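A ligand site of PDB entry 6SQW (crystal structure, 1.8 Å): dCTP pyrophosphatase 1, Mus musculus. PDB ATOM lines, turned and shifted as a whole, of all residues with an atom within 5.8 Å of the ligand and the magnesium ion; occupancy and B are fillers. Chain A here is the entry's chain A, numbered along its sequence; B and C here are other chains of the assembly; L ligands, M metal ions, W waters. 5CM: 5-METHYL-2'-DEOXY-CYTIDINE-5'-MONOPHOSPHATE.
The side-chain carboxylate of Asp 98 lies within hydrogen-bond range of an oxygen (O3') of the ligand (2.7 Å).
An oxygen (OP2) of the ligand lies within hydrogen-bond range of the side-chain hydroxyl (OH) of Tyr 129 of chain B (2.6 Å).
NE2 of His 38 is in hydrogen-bond range of O2 of the ligand.
The side-chain amide nitrogen of Asn 125 of chain B lies within hydrogen-bond range of an oxygen (O3') of the ligand (2.8 Å).
NH1 of Arg 128 of chain B lies within salt-bridge range of OP2 of the ligand (2.9 Å).
A ring nitrogen (NE2) of His 51 lies within hydrogen-bond range of a nitrogen (N3) of the ligand (2.9 Å).
The side-chain carboxylate of Asp 98 is in salt-bridge range of the side-chain amino group of Lys 121 of chain B (2.7 Å).
OD1 of Asn 125 of chain B is in hydrogen-bond range of NH2 of Arg 128 of chain B, at 2.9 Å.
OD1 of Asn 125 of chain B lies within hydrogen-bond range of NZ of Lys 121 of chain B, 2.9 Å away.
SD of Met 122 of chain B sits at hydrogen-bond distance from ND2 of Asn 125 of chain B (3.6 Å).
The indole nitrogen of Trp 73 of chain C sits close to the side-chain amide nitrogen of Gln 72 of chain C, at 3.3 Å.
The side-chain hydroxyl of Tyr 102 sits close to a nitrogen (N1) of the ligand (3.5 Å).
Residues that only touch the ligand: Phe 41, Trp 47, Ile 101, Lys 121 of chain B and Trp 73 of chain C.
Of the 20 residues printed, 12 come within 4 Å of the ligand.
The nearest printed residue that does not touch the ligand is Glu 63 (4.01 Å).
Within 4 Å of the magnesium ion: Glu 63, Glu 66, Glu 95 and Asp 98.
The nearest printed residue that does not touch the magnesium ion is Lys 121 of chain B (4.9 Å).
The magnesium ion is bound by the side-chain carboxylate of Glu 63 (2.0 Å), the side-chain carboxylate of Glu 66 (2.1 Å), the side-chain carboxylate of Glu 95 (2.1 Å), water W8 (2.1 Å), water W1 (2.1 Å) and the side-chain carboxylate of Asp 98 (2.1 Å).
The magnesium ion has six donor atoms within binding distance.
Water W1 lies within hydrogen-bond range of OE2 of Glu 63 (2.6 Å) and OP3 of the ligand (2.7 Å).
Water W4 lies within hydrogen-bond range of OP3 of the ligand, NZ of Lys 121 of chain B and NH2 of Arg 128 of chain B.
Water W2 lies within hydrogen-bond range of OP1 of the ligand, OH of Tyr 102, OE2 of Glu 63 and NE2 of Gln 72 of chain C.
Water W7 lies within hydrogen-bond range of an oxygen (OP3) of the ligand (2.8 Å) and the side-chain carboxylate of Glu 66 (3.3 Å).
Water W6 lies within hydrogen-bond range of NE1 of Trp 73 of chain C (2.9 Å) and OP1 of the ligand (2.9 Å).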
ATOM      1  N   HIS A  38      11.358 -13.240 -12.544  1.00  0.00           N
ATOM      2  CA  HIS A  38      10.058 -13.669 -13.004  1.00  0.00           C
ATOM      3  C   HIS A  38       9.251 -12.485 -13.563  1.00  0.00           C
ATOM      4  O   HIS A  38       8.613 -12.613 -14.610  1.00  0.00           O
ATOM      5  CB  HIS A  38       9.260 -14.411 -11.917  1.00  0.00           C
ATOM      6  CG  HIS A  38       7.955 -14.915 -12.407  1.00  0.00           C
ATOM      7  ND1 HIS A  38       6.772 -14.274 -12.136  1.00  0.00           N
ATOM      8  CD2 HIS A  38       7.655 -15.918 -13.272  1.00  0.00           C
ATOM      9  CE1 HIS A  38       5.789 -14.905 -12.738  1.00  0.00           C
ATOM     10  NE2 HIS A  38       6.301 -15.904 -13.451  1.00  0.00           N
ATOM     11  N   PHE A  41      10.510 -11.741 -17.032  1.00  0.00           N
ATOM     12  CA  PHE A  41      10.018 -12.795 -17.886  1.00  0.00           C
ATOM     13  C   PHE A  41       8.571 -12.582 -18.276  1.00  0.00           C
ATOM     14  O   PHE A  41       8.200 -12.698 -19.435  1.00  0.00           O
ATOM     15  CB  PHE A  41      10.234 -14.150 -17.129  1.00  0.00           C
ATOM     16  CG  PHE A  41       9.579 -15.315 -17.772  1.00  0.00           C
ATOM     17  CD1 PHE A  41      10.195 -15.996 -18.801  1.00  0.00           C
ATOM     18  CD2 PHE A  41       8.333 -15.761 -17.304  1.00  0.00           C
ATOM     19  CE1 PHE A  41       9.576 -17.071 -19.400  1.00  0.00           C
ATOM     20  CE2 PHE A  41       7.716 -16.847 -17.923  1.00  0.00           C
ATOM     21  CZ  PHE A  41       8.355 -17.511 -18.949  1.00  0.00           C
ATOM     22  N   TRP A  47       2.416 -11.078 -19.987  1.00  0.00           N
ATOM     23  CA  TRP A  47       1.681 -12.108 -19.243  1.00  0.00           C
ATOM     24  C   TRP A  47       1.058 -11.660 -17.908  1.00  0.00           C
ATOM     25  O   TRP A  47       0.374 -12.465 -17.265  1.00  0.00           O
ATOM     26  CB  TRP A  47       2.592 -13.315 -19.075  1.00  0.00           C
ATOM     27  CG  TRP A  47       2.635 -14.194 -20.279  1.00  0.00           C
ATOM     28  CD1 TRP A  47       1.968 -14.026 -21.469  1.00  0.00           C
ATOM     29  CD2 TRP A  47       3.389 -15.403 -20.410  1.00  0.00           C
ATOM     30  NE1 TRP A  47       2.266 -15.060 -22.321  1.00  0.00           N
ATOM     31  CE2 TRP A  47       3.120 -15.919 -21.696  1.00  0.00           C
ATOM     32  CE3 TRP A  47       4.222 -16.123 -19.555  1.00  0.00           C
ATOM     33  CZ2 TRP A  47       3.690 -17.113 -22.156  1.00  0.00           C
ATOM     34  CZ3 TRP A  47       4.817 -17.277 -20.021  1.00  0.00           C
ATOM     35  CH2 TRP A  47       4.541 -17.772 -21.309  1.00  0.00           C
ATOM     36  N   PHE A  50      -2.387 -12.806 -17.054  1.00  0.00           N
ATOM     37  CA  PHE A  50      -2.541 -14.176 -16.653  1.00  0.00           C
ATOM     38  C   PHE A  50      -2.072 -14.386 -15.211  1.00  0.00           C
ATOM     39  O   PHE A  50      -2.337 -15.420 -14.646  1.00  0.00           O
ATOM     40  CB  PHE A  50      -1.794 -15.132 -17.548  1.00  0.00           C
ATOM     41  CG  PHE A  50      -2.267 -15.116 -18.953  1.00  0.00           C
ATOM     42  CD1 PHE A  50      -3.418 -15.806 -19.318  1.00  0.00           C
ATOM     43  CD2 PHE A  50      -1.544 -14.421 -19.948  1.00  0.00           C
ATOM     44  CE1 PHE A  50      -3.866 -15.799 -20.654  1.00  0.00           C
ATOM     45  CE2 PHE A  50      -1.985 -14.401 -21.270  1.00  0.00           C
ATOM     46  CZ  PHE A  50      -3.149 -15.088 -21.617  1.00  0.00           C
ATOM     47  N   HIS A  51      -1.410 -13.409 -14.599  1.00  0.00           N
ATOM     48  CA  HIS A  51      -0.776 -13.582 -13.317  1.00  0.00           C
ATOM     49  C   HIS A  51      -1.550 -12.928 -12.185  1.00  0.00           C
ATOM     50  O   HIS A  51      -0.957 -12.404 -11.252  1.00  0.00           O
ATOM     51  CB  HIS A  51       0.695 -13.085 -13.391  1.00  0.00           C
ATOM     52  CG  HIS A  51       1.573 -13.965 -14.234  1.00  0.00           C
ATOM     53  ND1 HIS A  51       2.863 -13.638 -14.570  1.00  0.00           N
ATOM     54  CD2 HIS A  51       1.341 -15.170 -14.800  1.00  0.00           C
ATOM     55  CE1 HIS A  51       3.389 -14.619 -15.292  1.00  0.00           C
ATOM     56  NE2 HIS A  51       2.472 -15.556 -15.455  1.00  0.00           N
ATOM     57  N   GLU A  63       1.818 -27.257  -9.885  1.00  0.00           N
ATOM     58  CA  GLU A  63       3.217 -27.610  -9.718  1.00  0.00           C
ATOM     59  C   GLU A  63       3.482 -28.510  -8.508  1.00  0.00           C
ATOM     60  O   GLU A  63       4.306 -29.414  -8.564  1.00  0.00           O
ATOM     61  CB  GLU A  63       4.084 -26.352  -9.611  1.00  0.00           C
ATOM     62  CG  GLU A  63       3.939 -25.428 -10.799  1.00  0.00           C
ATOM     63  CD  GLU A  63       4.303 -25.993 -12.117  1.00  0.00           C
ATOM     64  OE1 GLU A  63       4.996 -27.058 -12.163  1.00  0.00           O
ATOM     65  OE2 GLU A  63       3.936 -25.342 -13.162  1.00  0.00           O
ATOM     66  N   GLU A  66       2.792 -31.860  -9.775  1.00  0.00           N
ATOM     67  CA  GLU A  66       3.883 -32.445 -10.517  1.00  0.00           C
ATOM     68  C   GLU A  66       4.998 -32.937  -9.591  1.00  0.00           C
ATOM     69  O   GLU A  66       5.589 -33.986  -9.833  1.00  0.00           O
ATOM     70  CB  GLU A  66       4.453 -31.459 -11.531  1.00  0.00           C
ATOM     71  CG  GLU A  66       3.529 -31.315 -12.705  1.00  0.00           C
ATOM     72  CD  GLU A  66       4.074 -30.434 -13.842  1.00  0.00           C
ATOM     73  OE1 GLU A  66       3.900 -30.904 -14.957  1.00  0.00           O
ATOM     74  OE2 GLU A  66       4.637 -29.337 -13.655  1.00  0.00           O
ATOM     75  N   GLU A  94      13.400 -29.253 -11.310  1.00  0.00           N
ATOM     76  CA  GLU A  94      12.518 -28.448 -12.102  1.00  0.00           C
ATOM     77  C   GLU A  94      11.195 -28.159 -11.380  1.00  0.00           C
ATOM     78  O   GLU A  94      10.736 -27.011 -11.380  1.00  0.00           O
ATOM     79  CB  GLU A  94      12.207 -29.115 -13.461  1.00  0.00           C
ATOM     80  CG  GLU A  94      13.369 -29.066 -14.446  1.00  0.00           C
ATOM     81  CD  GLU A  94      13.279 -30.175 -15.489  1.00  0.00           C
ATOM     82  OE1 GLU A  94      12.171 -30.702 -15.721  1.00  0.00           O
ATOM     83  OE2 GLU A  94      14.326 -30.548 -16.101  1.00  0.00           O
ATOM     84  N   GLU A  95      10.606 -29.167 -10.755  1.00  0.00           N
ATOM     85  CA  GLU A  95       9.323 -28.974 -10.079  1.00  0.00           C
ATOM     86  C   GLU A  95       9.466 -28.233  -8.794  1.00  0.00           C
ATOM     87  O   GLU A  95       8.632 -27.401  -8.493  1.00  0.00           O
ATOM     88  CB  GLU A  95       8.592 -30.300  -9.871  1.00  0.00           C
ATOM     89  CG  GLU A  95       8.319 -31.093 -11.145  1.00  0.00           C
ATOM     90  CD  GLU A  95       7.786 -30.299 -12.329  1.00  0.00           C
ATOM     91  OE1 GLU A  95       7.117 -29.233 -12.195  1.00  0.00           O
ATOM     92  OE2 GLU A  95       7.994 -30.726 -13.452  1.00  0.00           O
ATOM     93  N   SER A  97      11.528 -25.956  -8.402  1.00  0.00           N
ATOM     94  CA  SER A  97      11.729 -24.599  -8.916  1.00  0.00           C
ATOM     95  C   SER A  97      10.399 -23.981  -9.362  1.00  0.00           C
ATOM     96  O   SER A  97      10.134 -22.837  -9.048  1.00  0.00           O
ATOM     97  CB  SER A  97      12.733 -24.595 -10.072  1.00  0.00           C
ATOM     98  OG  SER A  97      14.017 -25.050  -9.640  1.00  0.00           O
ATOM     99  N   ASP A  98       9.590 -24.731 -10.127  1.00  0.00           N
ATOM    100  CA  ASP A  98       8.258 -24.250 -10.531  1.00  0.00           C
ATOM    101  C   ASP A  98       7.426 -23.869  -9.323  1.00  0.00           C
ATOM    102  O   ASP A  98       6.768 -22.816  -9.354  1.00  0.00           O
ATOM    103  CB  ASP A  98       7.494 -25.257 -11.369  1.00  0.00           C
ATOM    104  CG  ASP A  98       7.992 -25.411 -12.770  1.00  0.00           C
ATOM    105  OD1 ASP A  98       8.641 -24.479 -13.297  1.00  0.00           O
ATOM    106  OD2 ASP A  98       7.698 -26.493 -13.332  1.00  0.00           O
ATOM    107  N   ILE A 101       8.875 -20.546  -8.009  1.00  0.00           N
ATOM    108  CA  ILE A 101       8.643 -19.447  -8.927  1.00  0.00           C
ATOM    109  C   ILE A 101       7.221 -18.873  -8.752  1.00  0.00           C
ATOM    110  O   ILE A 101       7.022 -17.635  -8.528  1.00  0.00           O
ATOM    111  CB  ILE A 101       8.944 -19.829 -10.382  1.00  0.00           C
ATOM    112  CG1 ILE A 101      10.453 -20.026 -10.558  1.00  0.00           C
ATOM    113  CG2 ILE A 101       8.434 -18.741 -11.329  1.00  0.00           C
ATOM    114  CD1 ILE A 101      10.829 -20.873 -11.736  1.00  0.00           C
ATOM    115  N   TYR A 102       6.233 -19.773  -8.756  1.00  0.00           N
ATOM    116  CA  TYR A 102       4.881 -19.312  -8.554  1.00  0.00           C
ATOM    117  C   TYR A 102       4.679 -18.776  -7.173  1.00  0.00           C
ATOM    118  O   TYR A 102       3.895 -17.861  -6.987  1.00  0.00           O
ATOM    119  CB  TYR A 102       3.856 -20.371  -8.913  1.00  0.00           C
ATOM    120  CG  TYR A 102       3.714 -20.573 -10.393  1.00  0.00           C
ATOM    121  CD1 TYR A 102       3.373 -19.528 -11.237  1.00  0.00           C
ATOM    122  CD2 TYR A 102       3.805 -21.840 -10.943  1.00  0.00           C
ATOM    123  CE1 TYR A 102       3.183 -19.742 -12.595  1.00  0.00           C
ATOM    124  CE2 TYR A 102       3.607 -22.059 -12.279  1.00  0.00           C
ATOM    125  CZ  TYR A 102       3.298 -21.015 -13.094  1.00  0.00           C
ATOM    126  OH  TYR A 102       3.119 -21.263 -14.411  1.00  0.00           O
ATOM    127  N   LYS B 121      15.685 -23.452 -14.343  1.00  0.00           N
ATOM    128  CA  LYS B 121      14.280 -23.561 -14.759  1.00  0.00           C
ATOM    129  C   LYS B 121      13.823 -22.318 -15.528  1.00  0.00           C
ATOM    130  O   LYS B 121      13.158 -22.460 -16.548  1.00  0.00           O
ATOM    131  CB  LYS B 121      13.344 -23.856 -13.583  1.00  0.00           C
ATOM    132  CG  LYS B 121      11.921 -24.254 -14.013  1.00  0.00           C
ATOM    133  CD  LYS B 121      11.949 -25.399 -15.022  1.00  0.00           C
ATOM    134  CE  LYS B 121      10.622 -26.100 -15.218  1.00  0.00           C
ATOM    135  NZ  LYS B 121       9.547 -25.217 -15.744  1.00  0.00           N
ATOM    136  N   MET B 122      14.217 -21.130 -15.054  1.00  0.00           N
ATOM    137  CA  MET B 122      13.932 -19.891 -15.772  1.00  0.00           C
ATOM    138  C   MET B 122      14.542 -19.908 -17.180  1.00  0.00           C
ATOM    139  O   MET B 122      13.867 -19.568 -18.164  1.00  0.00           O
ATOM    140  CB  MET B 122      14.348 -18.666 -14.952  1.00  0.00           C
ATOM    141  CG  MET B 122      13.392 -18.349 -13.783  1.00  0.00           C
ATOM    142  SD  MET B 122      11.692 -18.029 -14.322  1.00  0.00           S
ATOM    143  CE  MET B 122      11.968 -16.459 -15.141  1.00  0.00           C
ATOM    144  N   ASN B 125      12.367 -22.136 -19.109  1.00  0.00           N
ATOM    145  CA  ASN B 125      11.106 -21.413 -19.368  1.00  0.00           C
ATOM    146  C   ASN B 125      11.224 -20.451 -20.575  1.00  0.00           C
ATOM    147  O   ASN B 125      10.341 -20.410 -21.457  1.00  0.00           O
ATOM    148  CB  ASN B 125      10.665 -20.618 -18.139  1.00  0.00           C
ATOM    149  CG  ASN B 125      10.219 -21.505 -16.986  1.00  0.00           C
ATOM    150  OD1 ASN B 125       9.978 -22.698 -17.169  1.00  0.00           O
ATOM    151  ND2 ASN B 125      10.130 -20.927 -15.786  1.00  0.00           N
ATOM    152  N   ARG B 128      11.187 -22.595 -23.751  1.00  0.00           N
ATOM    153  CA  ARG B 128       9.885 -23.145 -24.056  1.00  0.00           C
ATOM    154  C   ARG B 128       8.916 -22.066 -24.526  1.00  0.00           C
ATOM    155  O   ARG B 128       8.042 -22.348 -25.286  1.00  0.00           O
ATOM    156  CB  ARG B 128       9.318 -23.978 -22.881  1.00  0.00           C
ATOM    157  CG  ARG B 128      10.107 -25.278 -22.670  1.00  0.00           C
ATOM    158  CD  ARG B 128       9.797 -26.138 -21.419  1.00  0.00           C
ATOM    159  NE  ARG B 128       9.461 -25.276 -20.303  1.00  0.00           N
ATOM    160  CZ  ARG B 128       8.216 -24.954 -19.939  1.00  0.00           C
ATOM    161  NH1 ARG B 128       7.143 -25.465 -20.579  1.00  0.00           N
ATOM    162  NH2 ARG B 128       8.048 -24.082 -18.899  1.00  0.00           N
ATOM    163  N   TYR B 129       9.108 -20.824 -24.076  1.00  0.00           N
ATOM    164  CA  TYR B 129       8.245 -19.696 -24.468  1.00  0.00           C
ATOM    165  C   TYR B 129       9.045 -18.491 -24.973  1.00  0.00           C
ATOM    166  O   TYR B 129       9.148 -17.480 -24.280  1.00  0.00           O
ATOM    167  CB  TYR B 129       7.407 -19.256 -23.267  1.00  0.00           C
ATOM    168  CG  TYR B 129       6.475 -20.347 -22.789  1.00  0.00           C
ATOM    169  CD1 TYR B 129       5.319 -20.644 -23.514  1.00  0.00           C
ATOM    170  CD2 TYR B 129       6.751 -21.074 -21.615  1.00  0.00           C
ATOM    171  CE1 TYR B 129       4.446 -21.625 -23.094  1.00  0.00           C
ATOM    172  CE2 TYR B 129       5.874 -22.051 -21.182  1.00  0.00           C
ATOM    173  CZ  TYR B 129       4.721 -22.335 -21.935  1.00  0.00           C
ATOM    174  OH  TYR B 129       3.796 -23.294 -21.510  1.00  0.00           O
ATOM    175  N   GLN C  72      -6.076 -23.045 -14.441  1.00  0.00           N
ATOM    176  CA  GLN C  72      -5.134 -22.065 -13.925  1.00  0.00           C
ATOM    177  C   GLN C  72      -5.065 -20.760 -14.717  1.00  0.00           C
ATOM    178  O   GLN C  72      -4.857 -19.720 -14.132  1.00  0.00           O
ATOM    179  CB  GLN C  72      -3.747 -22.660 -13.746  1.00  0.00           C
ATOM    180  CG  GLN C  72      -2.974 -23.063 -14.992  1.00  0.00           C
ATOM    181  CD  GLN C  72      -1.697 -23.792 -14.606  1.00  0.00           C
ATOM    182  OE1 GLN C  72      -1.762 -24.788 -13.885  1.00  0.00           O
ATOM    183  NE2 GLN C  72      -0.556 -23.282 -15.010  1.00  0.00           N
ATOM    184  N   TRP C  73      -5.211 -20.848 -16.025  1.00  0.00           N
ATOM    185  CA  TRP C  73      -5.064 -19.685 -16.912  1.00  0.00           C
ATOM    186  C   TRP C  73      -6.418 -19.121 -17.355  1.00  0.00           C
ATOM    187  O   TRP C  73      -6.443 -18.230 -18.152  1.00  0.00           O
ATOM    188  CB  TRP C  73      -4.198 -20.042 -18.116  1.00  0.00           C
ATOM    189  CG  TRP C  73      -2.831 -20.494 -17.813  1.00  0.00           C
ATOM    190  CD1 TRP C  73      -2.200 -21.550 -18.373  1.00  0.00           C
ATOM    191  CD2 TRP C  73      -1.907 -19.918 -16.886  1.00  0.00           C
ATOM    192  NE1 TRP C  73      -0.935 -21.674 -17.860  1.00  0.00           N
ATOM    193  CE2 TRP C  73      -0.732 -20.690 -16.945  1.00  0.00           C
ATOM    194  CE3 TRP C  73      -1.955 -18.851 -15.983  1.00  0.00           C
ATOM    195  CZ2 TRP C  73       0.397 -20.414 -16.158  1.00  0.00           C
ATOM    196  CZ3 TRP C  73      -0.844 -18.602 -15.177  1.00  0.00           C
ATOM    197  CH2 TRP C  73       0.298 -19.373 -15.266  1.00  0.00           C
HETATM  198  N1  5CM L   1       5.302 -19.590 -16.570  1.00  0.00           N
HETATM  199  C2  5CM L   1       4.728 -18.405 -16.100  1.00  0.00           C
HETATM  200  N3  5CM L   1       3.535 -17.961 -16.582  1.00  0.00           N
HETATM  201  C4  5CM L   1       2.912 -18.611 -17.601  1.00  0.00           C
HETATM  202  C5  5CM L   1       3.498 -19.867 -18.113  1.00  0.00           C
HETATM  203  C5A 5CM L   1       2.853 -20.690 -19.237  1.00  0.00           C
HETATM  204  C6  5CM L   1       4.711 -20.276 -17.572  1.00  0.00           C
HETATM  205  O2  5CM L   1       5.319 -17.792 -15.175  1.00  0.00           O
HETATM  206  N4  5CM L   1       1.730 -18.148 -18.063  1.00  0.00           N
HETATM  207  C1' 5CM L   1       6.588 -20.034 -15.990  1.00  0.00           C
HETATM  208  C2' 5CM L   1       6.547 -20.324 -14.487  1.00  0.00           C
HETATM  209  C3' 5CM L   1       7.018 -21.797 -14.308  1.00  0.00           C
HETATM  210  C4' 5CM L   1       6.974 -22.373 -15.735  1.00  0.00           C
HETATM  211  O4' 5CM L   1       7.027 -21.245 -16.645  1.00  0.00           O
HETATM  212  O3' 5CM L   1       8.371 -21.865 -13.775  1.00  0.00           O
HETATM  213  C5' 5CM L   1       5.717 -23.192 -16.045  1.00  0.00           C
HETATM  214  O5' 5CM L   1       5.645 -23.586 -17.453  1.00  0.00           O
HETATM  215  P   5CM L   1       4.694 -24.828 -17.925  1.00  0.00           P
HETATM  216  OP1 5CM L   1       3.320 -24.592 -17.258  1.00  0.00           O
HETATM  217  OP2 5CM L   1       4.623 -24.684 -19.440  1.00  0.00           O
HETATM  218  OP3 5CM L   1       5.454 -26.070 -17.522  1.00  0.00           O
HETATM  219 MG    MG M   1       6.173 -27.964 -13.546  1.00  0.00          MG
HETATM  220  O   HOH W   1       5.084 -26.866 -15.001  1.00  0.00           O
HETATM  221  O   HOH W   2       2.304 -23.827 -14.870  1.00  0.00           O
HETATM  222  O   HOH W   3       2.134 -26.954 -16.812  1.00  0.00           O
HETATM  223  O   HOH W   4       7.925 -26.849 -17.307  1.00  0.00           O
HETATM  224  O   HOH W   5       3.249 -26.782 -20.781  1.00  0.00           O
HETATM  225  O   HOH W   6       0.925 -23.727 -18.601  1.00  0.00           O
HETATM  226  O   HOH W   7       4.650 -28.754 -17.310  1.00  0.00           O
HETATM  227  O   HOH W   8       7.026 -28.846 -15.226  1.00  0.00           O
